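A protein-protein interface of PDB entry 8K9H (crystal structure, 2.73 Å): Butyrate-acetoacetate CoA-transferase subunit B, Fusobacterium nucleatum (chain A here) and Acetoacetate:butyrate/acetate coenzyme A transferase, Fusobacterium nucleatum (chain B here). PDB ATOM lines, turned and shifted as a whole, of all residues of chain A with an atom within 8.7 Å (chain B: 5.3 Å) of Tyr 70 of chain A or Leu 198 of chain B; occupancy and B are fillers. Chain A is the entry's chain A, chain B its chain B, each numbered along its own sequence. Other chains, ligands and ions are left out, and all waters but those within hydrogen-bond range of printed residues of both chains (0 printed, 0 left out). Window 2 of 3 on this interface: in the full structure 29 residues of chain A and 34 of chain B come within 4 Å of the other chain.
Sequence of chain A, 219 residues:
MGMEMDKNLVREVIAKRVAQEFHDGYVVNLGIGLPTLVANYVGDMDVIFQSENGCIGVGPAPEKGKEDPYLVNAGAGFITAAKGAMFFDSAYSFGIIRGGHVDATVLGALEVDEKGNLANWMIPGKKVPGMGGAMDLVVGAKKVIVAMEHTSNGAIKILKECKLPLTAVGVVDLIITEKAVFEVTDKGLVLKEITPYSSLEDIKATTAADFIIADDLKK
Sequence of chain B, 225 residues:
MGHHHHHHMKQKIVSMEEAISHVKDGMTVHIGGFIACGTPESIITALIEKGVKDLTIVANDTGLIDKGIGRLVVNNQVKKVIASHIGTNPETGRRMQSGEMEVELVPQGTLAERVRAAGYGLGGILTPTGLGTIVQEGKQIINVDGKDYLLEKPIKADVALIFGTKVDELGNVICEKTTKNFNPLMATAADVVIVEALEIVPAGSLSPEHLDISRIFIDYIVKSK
The backbone carbonyl oxygen (O) of Pro 69 of chain A sits at hydrogen-bond distance from the side-chain sulfur (SG) of Cys 37 of chain B, at 3.7 Å. The backbone NH of Thr 178 of chain B is in hydrogen-bond range of the backbone carbonyl oxygen of Tyr 70 of chain A, 3.0 Å away. The side-chain hydroxyl (OG1) of Thr 178 of chain B is in hydrogen-bond range of the backbone NH (N) of Val 72 of chain A (3.1 Å).
ND2 of Asn 53 of chain A is in hydrogen-bond range of O of Val 72 of chain A (3.0 Å). The backbone NH (N) of Tyr 70 of chain A sits at hydrogen-bond distance from the side-chain carboxylate (OD1) of Asp 68 of chain A, at 2.9 Å. The side-chain sulfur of Cys 37 of chain B is in hydrogen-bond range of the backbone carbonyl oxygen of Thr 178 of chain B (3.6 Å). The backbone carbonyl oxygen of Gly 164 of chain B lies within hydrogen-bond range of the backbone NH of Leu 198 of chain B, 2.8 Å away. The backbone NH (N) of Glu 176 of chain B is in hydrogen-bond range of the side-chain hydroxyl (OG1) of Thr 165 of chain B (3.3 Å). The backbone carbonyl oxygen (O) of Glu 176 of chain B sits at hydrogen-bond distance from the side-chain hydroxyl (OG1) of Thr 179 of chain B, at 2.6 Å.
Asn 53 of chain A touches Thr 178 of chain B (ND2 to CB, 3.5 Å). OD2 of Asp 68 of chain A touches CD of Lys 177 of chain B, 3.5 Å away. Tyr 70 of chain A touches Glu 176 of chain B. CB of Lys 177 of chain B touches O of Tyr 70 of chain A (3.1 Å). Tyr 70 of chain A touches Thr 179 of chain B. Tyr 70 of chain A touches Leu 198 of chain B (OH to CD2, 3.3 Å). CB of Lys 177 of chain B touches CB of Leu 71 of chain A (3.8 Å). Thr 178 of chain B touches Leu 71 of chain A. Lys 177 of chain B touches Phe 87 of chain A.
Printed residues of chain B within 4 Å of Pro 69 of chain A: Cys 37. Printed residues of chain B within 4 Å of Tyr 70 of chain A: Glu 176 (3.9 Å), Lys 177 (3.1 Å), Thr 178 (3.0 Å), Thr 179 (3.8 Å) and Leu 198 (3.3 Å). Printed residues of chain B within 4 Å of Val 72 of chain A: Thr 178 (3.1 Å). Of the printed residues of chain B, Phe 87 of chain A touches Lys 177 (3.5 Å). Of the printed residues of chain A, Thr 179 of chain B touches Tyr 70 (3.8 Å). No residue of chain A comes within 4 Å of Ala 197 of chain B. Of chain A, only Tyr 70 comes within 4 Å of Leu 198 of chain B.
Of the 13 printed residues of chain A, 7 touch a printed residue of chain B. Among the printed residues, 12 pairs touch across the chains. Among the printed residues, no Asp or Glu carboxylate lies within 4 Å of a Lys or Arg side-chain nitrogen of the other chain.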
ATOM      1  N   ASN A  53     -37.572  -4.418  -2.718  1.00  0.00           N
ATOM      2  CA  ASN A  53     -36.530  -3.814  -3.550  1.00  0.00           C
ATOM      3  C   ASN A  53     -35.127  -4.292  -3.193  1.00  0.00           C
ATOM      4  O   ASN A  53     -34.161  -3.907  -3.863  1.00  0.00           O
ATOM      5  CB  ASN A  53     -36.601  -2.285  -3.492  1.00  0.00           C
ATOM      6  CG  ASN A  53     -36.344  -1.736  -2.101  1.00  0.00           C
ATOM      7  OD1 ASN A  53     -36.948  -2.182  -1.127  1.00  0.00           O
ATOM      8  ND2 ASN A  53     -35.447  -0.750  -2.005  1.00  0.00           N
ATOM      9  N   GLU A  67     -29.178   9.739   6.489  1.00  0.00           N
ATOM     10  CA  GLU A  67     -30.287   9.686   5.536  1.00  0.00           C
ATOM     11  C   GLU A  67     -29.738   9.414   4.122  1.00  0.00           C
ATOM     12  O   GLU A  67     -29.509  10.341   3.328  1.00  0.00           O
ATOM     13  CB  GLU A  67     -31.129  10.981   5.572  1.00  0.00           C
ATOM     14  N   ASP A  68     -29.549   8.114   3.831  1.00  0.00           N
ATOM     15  CA  ASP A  68     -28.924   7.640   2.592  1.00  0.00           C
ATOM     16  C   ASP A  68     -29.983   7.438   1.519  1.00  0.00           C
ATOM     17  O   ASP A  68     -30.921   6.662   1.734  1.00  0.00           O
ATOM     18  CB  ASP A  68     -28.190   6.322   2.841  1.00  0.00           C
ATOM     19  CG  ASP A  68     -27.227   5.951   1.717  1.00  0.00           C
ATOM     20  OD1 ASP A  68     -27.381   6.498   0.606  1.00  0.00           O
ATOM     21  OD2 ASP A  68     -26.310   5.115   1.951  1.00  0.00           O
ATOM     22  N   PRO A  69     -29.878   8.084   0.357  1.00  0.00           N
ATOM     23  CA  PRO A  69     -30.871   7.864  -0.700  1.00  0.00           C
ATOM     24  C   PRO A  69     -30.609   6.627  -1.555  1.00  0.00           C
ATOM     25  O   PRO A  69     -31.440   6.303  -2.412  1.00  0.00           O
ATOM     26  CB  PRO A  69     -30.750   9.144  -1.532  1.00  0.00           C
ATOM     27  CG  PRO A  69     -29.299   9.474  -1.446  1.00  0.00           C
ATOM     28  CD  PRO A  69     -28.854   9.063  -0.053  1.00  0.00           C
ATOM     29  N   TYR A  70     -29.480   5.939  -1.361  1.00  0.00           N
ATOM     30  CA  TYR A  70     -29.173   4.681  -2.030  1.00  0.00           C
ATOM     31  C   TYR A  70     -29.604   3.467  -1.214  1.00  0.00           C
ATOM     32  O   TYR A  70     -29.264   2.328  -1.573  1.00  0.00           O
ATOM     33  CB  TYR A  70     -27.672   4.593  -2.324  1.00  0.00           C
ATOM     34  CG  TYR A  70     -27.182   5.598  -3.335  1.00  0.00           C
ATOM     35  CD1 TYR A  70     -28.034   6.111  -4.303  1.00  0.00           C
ATOM     36  CD2 TYR A  70     -25.863   6.034  -3.324  1.00  0.00           C
ATOM     37  CE1 TYR A  70     -27.585   7.033  -5.234  1.00  0.00           C
ATOM     38  CE2 TYR A  70     -25.407   6.960  -4.246  1.00  0.00           C
ATOM     39  CZ  TYR A  70     -26.267   7.457  -5.196  1.00  0.00           C
ATOM     40  OH  TYR A  70     -25.816   8.376  -6.118  1.00  0.00           O
ATOM     41  N   LEU A  71     -30.334   3.684  -0.119  1.00  0.00           N
ATOM     42  CA  LEU A  71     -30.793   2.600   0.751  1.00  0.00           C
ATOM     43  C   LEU A  71     -32.189   2.983   1.237  1.00  0.00           C
ATOM     44  O   LEU A  71     -32.326   3.750   2.192  1.00  0.00           O
ATOM     45  CB  LEU A  71     -29.817   2.373   1.904  1.00  0.00           C
ATOM     46  CG  LEU A  71     -30.282   1.595   3.124  1.00  0.00           C
ATOM     47  CD1 LEU A  71     -30.770   0.226   2.712  1.00  0.00           C
ATOM     48  CD2 LEU A  71     -29.131   1.479   4.082  1.00  0.00           C
ATOM     49  N   VAL A  72     -33.219   2.472   0.559  1.00  0.00           N
ATOM     50  CA  VAL A  72     -34.609   2.761   0.881  1.00  0.00           C
ATOM     51  C   VAL A  72     -35.415   1.462   0.896  1.00  0.00           C
ATOM     52  O   VAL A  72     -34.875   0.369   0.773  1.00  0.00           O
ATOM     53  CB  VAL A  72     -35.228   3.782  -0.090  1.00  0.00           C
ATOM     54  CG1 VAL A  72     -34.674   5.149   0.206  1.00  0.00           C
ATOM     55  CG2 VAL A  72     -34.946   3.386  -1.531  1.00  0.00           C
ATOM     56  N   ASN A  73     -36.721   1.600   1.067  1.00  0.00           N
ATOM     57  CA  ASN A  73     -37.621   0.467   1.153  1.00  0.00           C
ATOM     58  C   ASN A  73     -38.526   0.430  -0.080  1.00  0.00           C
ATOM     59  O   ASN A  73     -38.348   1.212  -1.029  1.00  0.00           O
ATOM     60  CB  ASN A  73     -38.425   0.542   2.450  1.00  0.00           C
ATOM     61  CG  ASN A  73     -39.138   1.867   2.607  1.00  0.00           C
ATOM     62  OD1 ASN A  73     -39.495   2.504   1.625  1.00  0.00           O
ATOM     63  ND2 ASN A  73     -39.342   2.290   3.844  1.00  0.00           N
ATOM     64  N   ALA A  76     -39.887   3.826  -1.195  1.00  0.00           N
ATOM     65  CA  ALA A  76     -38.962   4.924  -1.447  1.00  0.00           C
ATOM     66  C   ALA A  76     -38.477   5.656  -0.197  1.00  0.00           C
ATOM     67  O   ALA A  76     -37.649   6.560  -0.333  1.00  0.00           O
ATOM     68  CB  ALA A  76     -39.558   5.964  -2.404  1.00  0.00           C
ATOM     69  N   GLY A  77     -38.948   5.305   1.005  1.00  0.00           N
ATOM     70  CA  GLY A  77     -38.516   6.005   2.211  1.00  0.00           C
ATOM     71  C   GLY A  77     -37.169   5.525   2.736  1.00  0.00           C
ATOM     72  O   GLY A  77     -36.782   4.367   2.574  1.00  0.00           O
ATOM     73  N   PHE A  78     -36.450   6.434   3.406  1.00  0.00           N
ATOM     74  CA  PHE A  78     -35.106   6.118   3.893  1.00  0.00           C
ATOM     75  C   PHE A  78     -35.143   5.077   5.010  1.00  0.00           C
ATOM     76  O   PHE A  78     -35.947   5.171   5.947  1.00  0.00           O
ATOM     77  CB  PHE A  78     -34.405   7.376   4.394  1.00  0.00           C
ATOM     78  CG  PHE A  78     -34.414   8.496   3.419  1.00  0.00           C
ATOM     79  CD1 PHE A  78     -33.502   8.526   2.381  1.00  0.00           C
ATOM     80  CD2 PHE A  78     -35.337   9.524   3.532  1.00  0.00           C
ATOM     81  CE1 PHE A  78     -33.502   9.562   1.467  1.00  0.00           C
ATOM     82  CE2 PHE A  78     -35.346  10.571   2.624  1.00  0.00           C
ATOM     83  CZ  PHE A  78     -34.428  10.589   1.591  1.00  0.00           C
ATOM     84  N   ILE A  79     -34.250   4.092   4.909  1.00  0.00           N
ATOM     85  CA  ILE A  79     -34.102   3.022   5.881  1.00  0.00           C
ATOM     86  C   ILE A  79     -32.618   2.864   6.216  1.00  0.00           C
ATOM     87  O   ILE A  79     -31.753   3.590   5.711  1.00  0.00           O
ATOM     88  CB  ILE A  79     -34.694   1.681   5.386  1.00  0.00           C
ATOM     89  CG1 ILE A  79     -33.862   1.105   4.238  1.00  0.00           C
ATOM     90  CG2 ILE A  79     -36.146   1.829   4.964  1.00  0.00           C
ATOM     91  CD1 ILE A  79     -34.081  -0.364   4.034  1.00  0.00           C
ATOM     92  N   PHE A  87     -27.924  -7.453   1.159  1.00  0.00           N
ATOM     93  CA  PHE A  87     -28.424  -6.675   0.039  1.00  0.00           C
ATOM     94  C   PHE A  87     -28.343  -7.511  -1.236  1.00  0.00           C
ATOM     95  O   PHE A  87     -27.328  -8.170  -1.487  1.00  0.00           O
ATOM     96  CB  PHE A  87     -27.595  -5.411  -0.129  1.00  0.00           C
ATOM     97  CG  PHE A  87     -27.882  -4.351   0.880  1.00  0.00           C
ATOM     98  CD1 PHE A  87     -29.193  -3.999   1.187  1.00  0.00           C
ATOM     99  CD2 PHE A  87     -26.839  -3.685   1.510  1.00  0.00           C
ATOM    100  CE1 PHE A  87     -29.464  -3.002   2.113  1.00  0.00           C
ATOM    101  CE2 PHE A  87     -27.098  -2.684   2.434  1.00  0.00           C
ATOM    102  CZ  PHE A  87     -28.411  -2.339   2.736  1.00  0.00           C
ATOM    103  N   CYS B  37     -34.221   4.801  -7.442  1.00  0.00           N
ATOM    104  CA  CYS B  37     -33.072   4.363  -6.655  1.00  0.00           C
ATOM    105  C   CYS B  37     -32.269   3.362  -7.479  1.00  0.00           C
ATOM    106  O   CYS B  37     -32.630   2.184  -7.580  1.00  0.00           O
ATOM    107  CB  CYS B  37     -33.507   3.753  -5.330  1.00  0.00           C
ATOM    108  SG  CYS B  37     -32.059   3.184  -4.393  1.00  0.00           S
ATOM    109  N   PHE B 163     -26.827   1.324 -13.763  1.00  0.00           N
ATOM    110  CA  PHE B 163     -26.199   2.292 -12.871  1.00  0.00           C
ATOM    111  C   PHE B 163     -25.297   1.550 -11.898  1.00  0.00           C
ATOM    112  O   PHE B 163     -25.653   0.475 -11.416  1.00  0.00           O
ATOM    113  CB  PHE B 163     -27.275   3.098 -12.114  1.00  0.00           C
ATOM    114  CG  PHE B 163     -26.812   3.668 -10.794  1.00  0.00           C
ATOM    115  CD1 PHE B 163     -26.871   2.909  -9.619  1.00  0.00           C
ATOM    116  CD2 PHE B 163     -26.320   4.970 -10.719  1.00  0.00           C
ATOM    117  CE1 PHE B 163     -26.433   3.430  -8.412  1.00  0.00           C
ATOM    118  CE2 PHE B 163     -25.886   5.496  -9.508  1.00  0.00           C
ATOM    119  CZ  PHE B 163     -25.944   4.728  -8.355  1.00  0.00           C
ATOM    120  N   GLY B 164     -24.134   2.123 -11.602  1.00  0.00           N
ATOM    121  CA  GLY B 164     -23.265   1.548 -10.590  1.00  0.00           C
ATOM    122  C   GLY B 164     -22.612   2.558  -9.662  1.00  0.00           C
ATOM    123  O   GLY B 164     -21.979   3.511 -10.130  1.00  0.00           O
ATOM    124  N   THR B 165     -22.738   2.366  -8.342  1.00  0.00           N
ATOM    125  CA  THR B 165     -22.076   3.284  -7.413  1.00  0.00           C
ATOM    126  C   THR B 165     -20.560   3.247  -7.578  1.00  0.00           C
ATOM    127  O   THR B 165     -19.881   4.243  -7.308  1.00  0.00           O
ATOM    128  CB  THR B 165     -22.458   2.974  -5.957  1.00  0.00           C
ATOM    129  OG1 THR B 165     -22.295   1.579  -5.701  1.00  0.00           O
ATOM    130  CG2 THR B 165     -23.909   3.381  -5.650  1.00  0.00           C
ATOM    131  N   LYS B 166     -20.010   2.122  -8.026  1.00  0.00           N
ATOM    132  CA  LYS B 166     -18.606   2.054  -8.400  1.00  0.00           C
ATOM    133  C   LYS B 166     -18.448   1.124  -9.610  1.00  0.00           C
ATOM    134  O   LYS B 166     -19.111   0.088  -9.705  1.00  0.00           O
ATOM    135  CB  LYS B 166     -17.740   1.608  -7.199  1.00  0.00           C
ATOM    136  N   GLU B 176     -24.456  -0.651  -4.737  1.00  0.00           N
ATOM    137  CA  GLU B 176     -24.454  -0.727  -3.289  1.00  0.00           C
ATOM    138  C   GLU B 176     -25.859  -0.584  -2.736  1.00  0.00           C
ATOM    139  O   GLU B 176     -26.730   0.038  -3.350  1.00  0.00           O
ATOM    140  CB  GLU B 176     -23.574   0.366  -2.701  1.00  0.00           C
ATOM    141  CG  GLU B 176     -22.103   0.047  -2.701  1.00  0.00           C
ATOM    142  CD  GLU B 176     -21.287   1.086  -1.948  1.00  0.00           C
ATOM    143  OE1 GLU B 176     -21.886   2.064  -1.436  1.00  0.00           O
ATOM    144  OE2 GLU B 176     -20.047   0.922  -1.879  1.00  0.00           O
ATOM    145  N   LYS B 177     -26.058  -1.150  -1.548  1.00  0.00           N
ATOM    146  CA  LYS B 177     -27.297  -1.016  -0.775  1.00  0.00           C
ATOM    147  C   LYS B 177     -28.461  -1.426  -1.680  1.00  0.00           C
ATOM    148  O   LYS B 177     -28.400  -2.508  -2.283  1.00  0.00           O
ATOM    149  CB  LYS B 177     -27.357   0.390  -0.173  1.00  0.00           C
ATOM    150  CG  LYS B 177     -26.303   0.634   0.934  1.00  0.00           C
ATOM    151  CD  LYS B 177     -25.474   1.907   0.690  1.00  0.00           C
ATOM    152  CE  LYS B 177     -24.179   1.951   1.511  1.00  0.00           C
ATOM    153  N   THR B 178     -29.513  -0.619  -1.819  1.00  0.00           N
ATOM    154  CA  THR B 178     -30.662  -1.035  -2.617  1.00  0.00           C
ATOM    155  C   THR B 178     -30.634  -0.470  -4.040  1.00  0.00           C
ATOM    156  O   THR B 178     -31.690  -0.336  -4.670  1.00  0.00           O
ATOM    157  CB  THR B 178     -31.983  -0.659  -1.933  1.00  0.00           C
ATOM    158  OG1 THR B 178     -32.029   0.751  -1.677  1.00  0.00           O
ATOM    159  CG2 THR B 178     -32.125  -1.400  -0.633  1.00  0.00           C
ATOM    160  N   THR B 179     -29.452  -0.164  -4.577  1.00  0.00           N
ATOM    161  CA  THR B 179     -29.359   0.245  -5.974  1.00  0.00           C
ATOM    162  C   THR B 179     -29.193  -0.946  -6.902  1.00  0.00           C
ATOM    163  O   THR B 179     -28.916  -0.772  -8.088  1.00  0.00           O
ATOM    164  CB  THR B 179     -28.205   1.227  -6.185  1.00  0.00           C
ATOM    165  OG1 THR B 179     -26.955   0.590  -5.863  1.00  0.00           O
ATOM    166  CG2 THR B 179     -28.409   2.468  -5.327  1.00  0.00           C
ATOM    167  N   GLU B 196     -23.875   3.738 -16.164  1.00  0.00           N
ATOM    168  CA  GLU B 196     -23.517   5.073 -15.685  1.00  0.00           C
ATOM    169  C   GLU B 196     -22.876   4.936 -14.312  1.00  0.00           C
ATOM    170  O   GLU B 196     -23.541   4.551 -13.347  1.00  0.00           O
ATOM    171  CB  GLU B 196     -24.731   5.991 -15.592  1.00  0.00           C
ATOM    172  CG  GLU B 196     -24.444   7.194 -14.699  1.00  0.00           C
ATOM    173  CD  GLU B 196     -25.617   8.149 -14.568  1.00  0.00           C
ATOM    174  OE1 GLU B 196     -25.722   8.820 -13.511  1.00  0.00           O
ATOM    175  OE2 GLU B 196     -26.428   8.233 -15.520  1.00  0.00           O
ATOM    176  N   ALA B 197     -21.591   5.262 -14.220  1.00  0.00           N
ATOM    177  CA  ALA B 197     -20.841   5.080 -12.987  1.00  0.00           C
ATOM    178  C   ALA B 197     -20.906   6.338 -12.132  1.00  0.00           C
ATOM    179  O   ALA B 197     -20.751   7.461 -12.637  1.00  0.00           O
ATOM    180  CB  ALA B 197     -19.388   4.730 -13.280  1.00  0.00           C
ATOM    181  N   LEU B 198     -21.166   6.138 -10.841  1.00  0.00           N
ATOM    182  CA  LEU B 198     -21.011   7.212  -9.873  1.00  0.00           C
ATOM    183  C   LEU B 198     -19.547   7.585  -9.733  1.00  0.00           C
ATOM    184  O   LEU B 198     -19.186   8.768  -9.779  1.00  0.00           O
ATOM    185  CB  LEU B 198     -21.571   6.771  -8.530  1.00  0.00           C
ATOM    186  CG  LEU B 198     -22.190   7.898  -7.734  1.00  0.00           C
ATOM    187  CD1 LEU B 198     -23.327   8.536  -8.543  1.00  0.00           C
ATOM    188  CD2 LEU B 198     -22.657   7.353  -6.382  1.00  0.00           C
ATOM    189  N   GLU B 199     -18.694   6.573  -9.581  1.00  0.00           N
ATOM    190  CA  GLU B 199     -17.250   6.702  -9.485  1.00  0.00           C
ATOM    191  C   GLU B 199     -16.607   5.628 -10.356  1.00  0.00           C
ATOM    192  O   GLU B 199     -17.068   4.485 -10.389  1.00  0.00           O
ATOM    193  CB  GLU B 199     -16.803   6.575  -8.009  1.00  0.00           C
ATOM    194  CG  GLU B 199     -15.358   6.145  -7.775  1.00  0.00           C
ATOM    195  CD  GLU B 199     -15.129   5.671  -6.344  1.00  0.00           C
ATOM    196  OE1 GLU B 199     -13.954   5.564  -5.910  1.00  0.00           O
ATOM    197  OE2 GLU B 199     -16.139   5.400  -5.650  1.00  0.00           O
ATOM    198  N   ILE B 200     -15.553   5.995 -11.079  1.00  0.00           N
ATOM    199  CA  ILE B 200     -14.786   5.045 -11.883  1.00  0.00           C
ATOM    200  C   ILE B 200     -13.519   4.702 -11.094  1.00  0.00           C
ATOM    201  O   ILE B 200     -12.557   5.472 -11.072  1.00  0.00           O
ATOM    202  CB  ILE B 200     -14.469   5.601 -13.277  1.00  0.00           C
ATOM    203  CG1 ILE B 200     -15.751   5.831 -14.083  1.00  0.00           C
ATOM    204  CG2 ILE B 200     -13.578   4.658 -14.047  1.00  0.00           C
ATOM    205  CD1 ILE B 200     -15.513   6.191 -15.560  1.00  0.00           C
ATOM    206  N   SER B 224     -21.169  10.076 -14.204  1.00  0.00           N
ATOM    207  CA  SER B 224     -22.385  10.842 -13.962  1.00  0.00           C
ATOM    208  C   SER B 224     -22.118  12.332 -14.000  1.00  0.00           C
ATOM    209  O   SER B 224     -21.176  12.785 -13.369  1.00  0.00           O
ATOM    210  CB  SER B 224     -22.978  10.448 -12.620  1.00  0.00           C
ATOM    211  OG  SER B 224     -22.774   9.068 -12.403  1.00  0.00           O
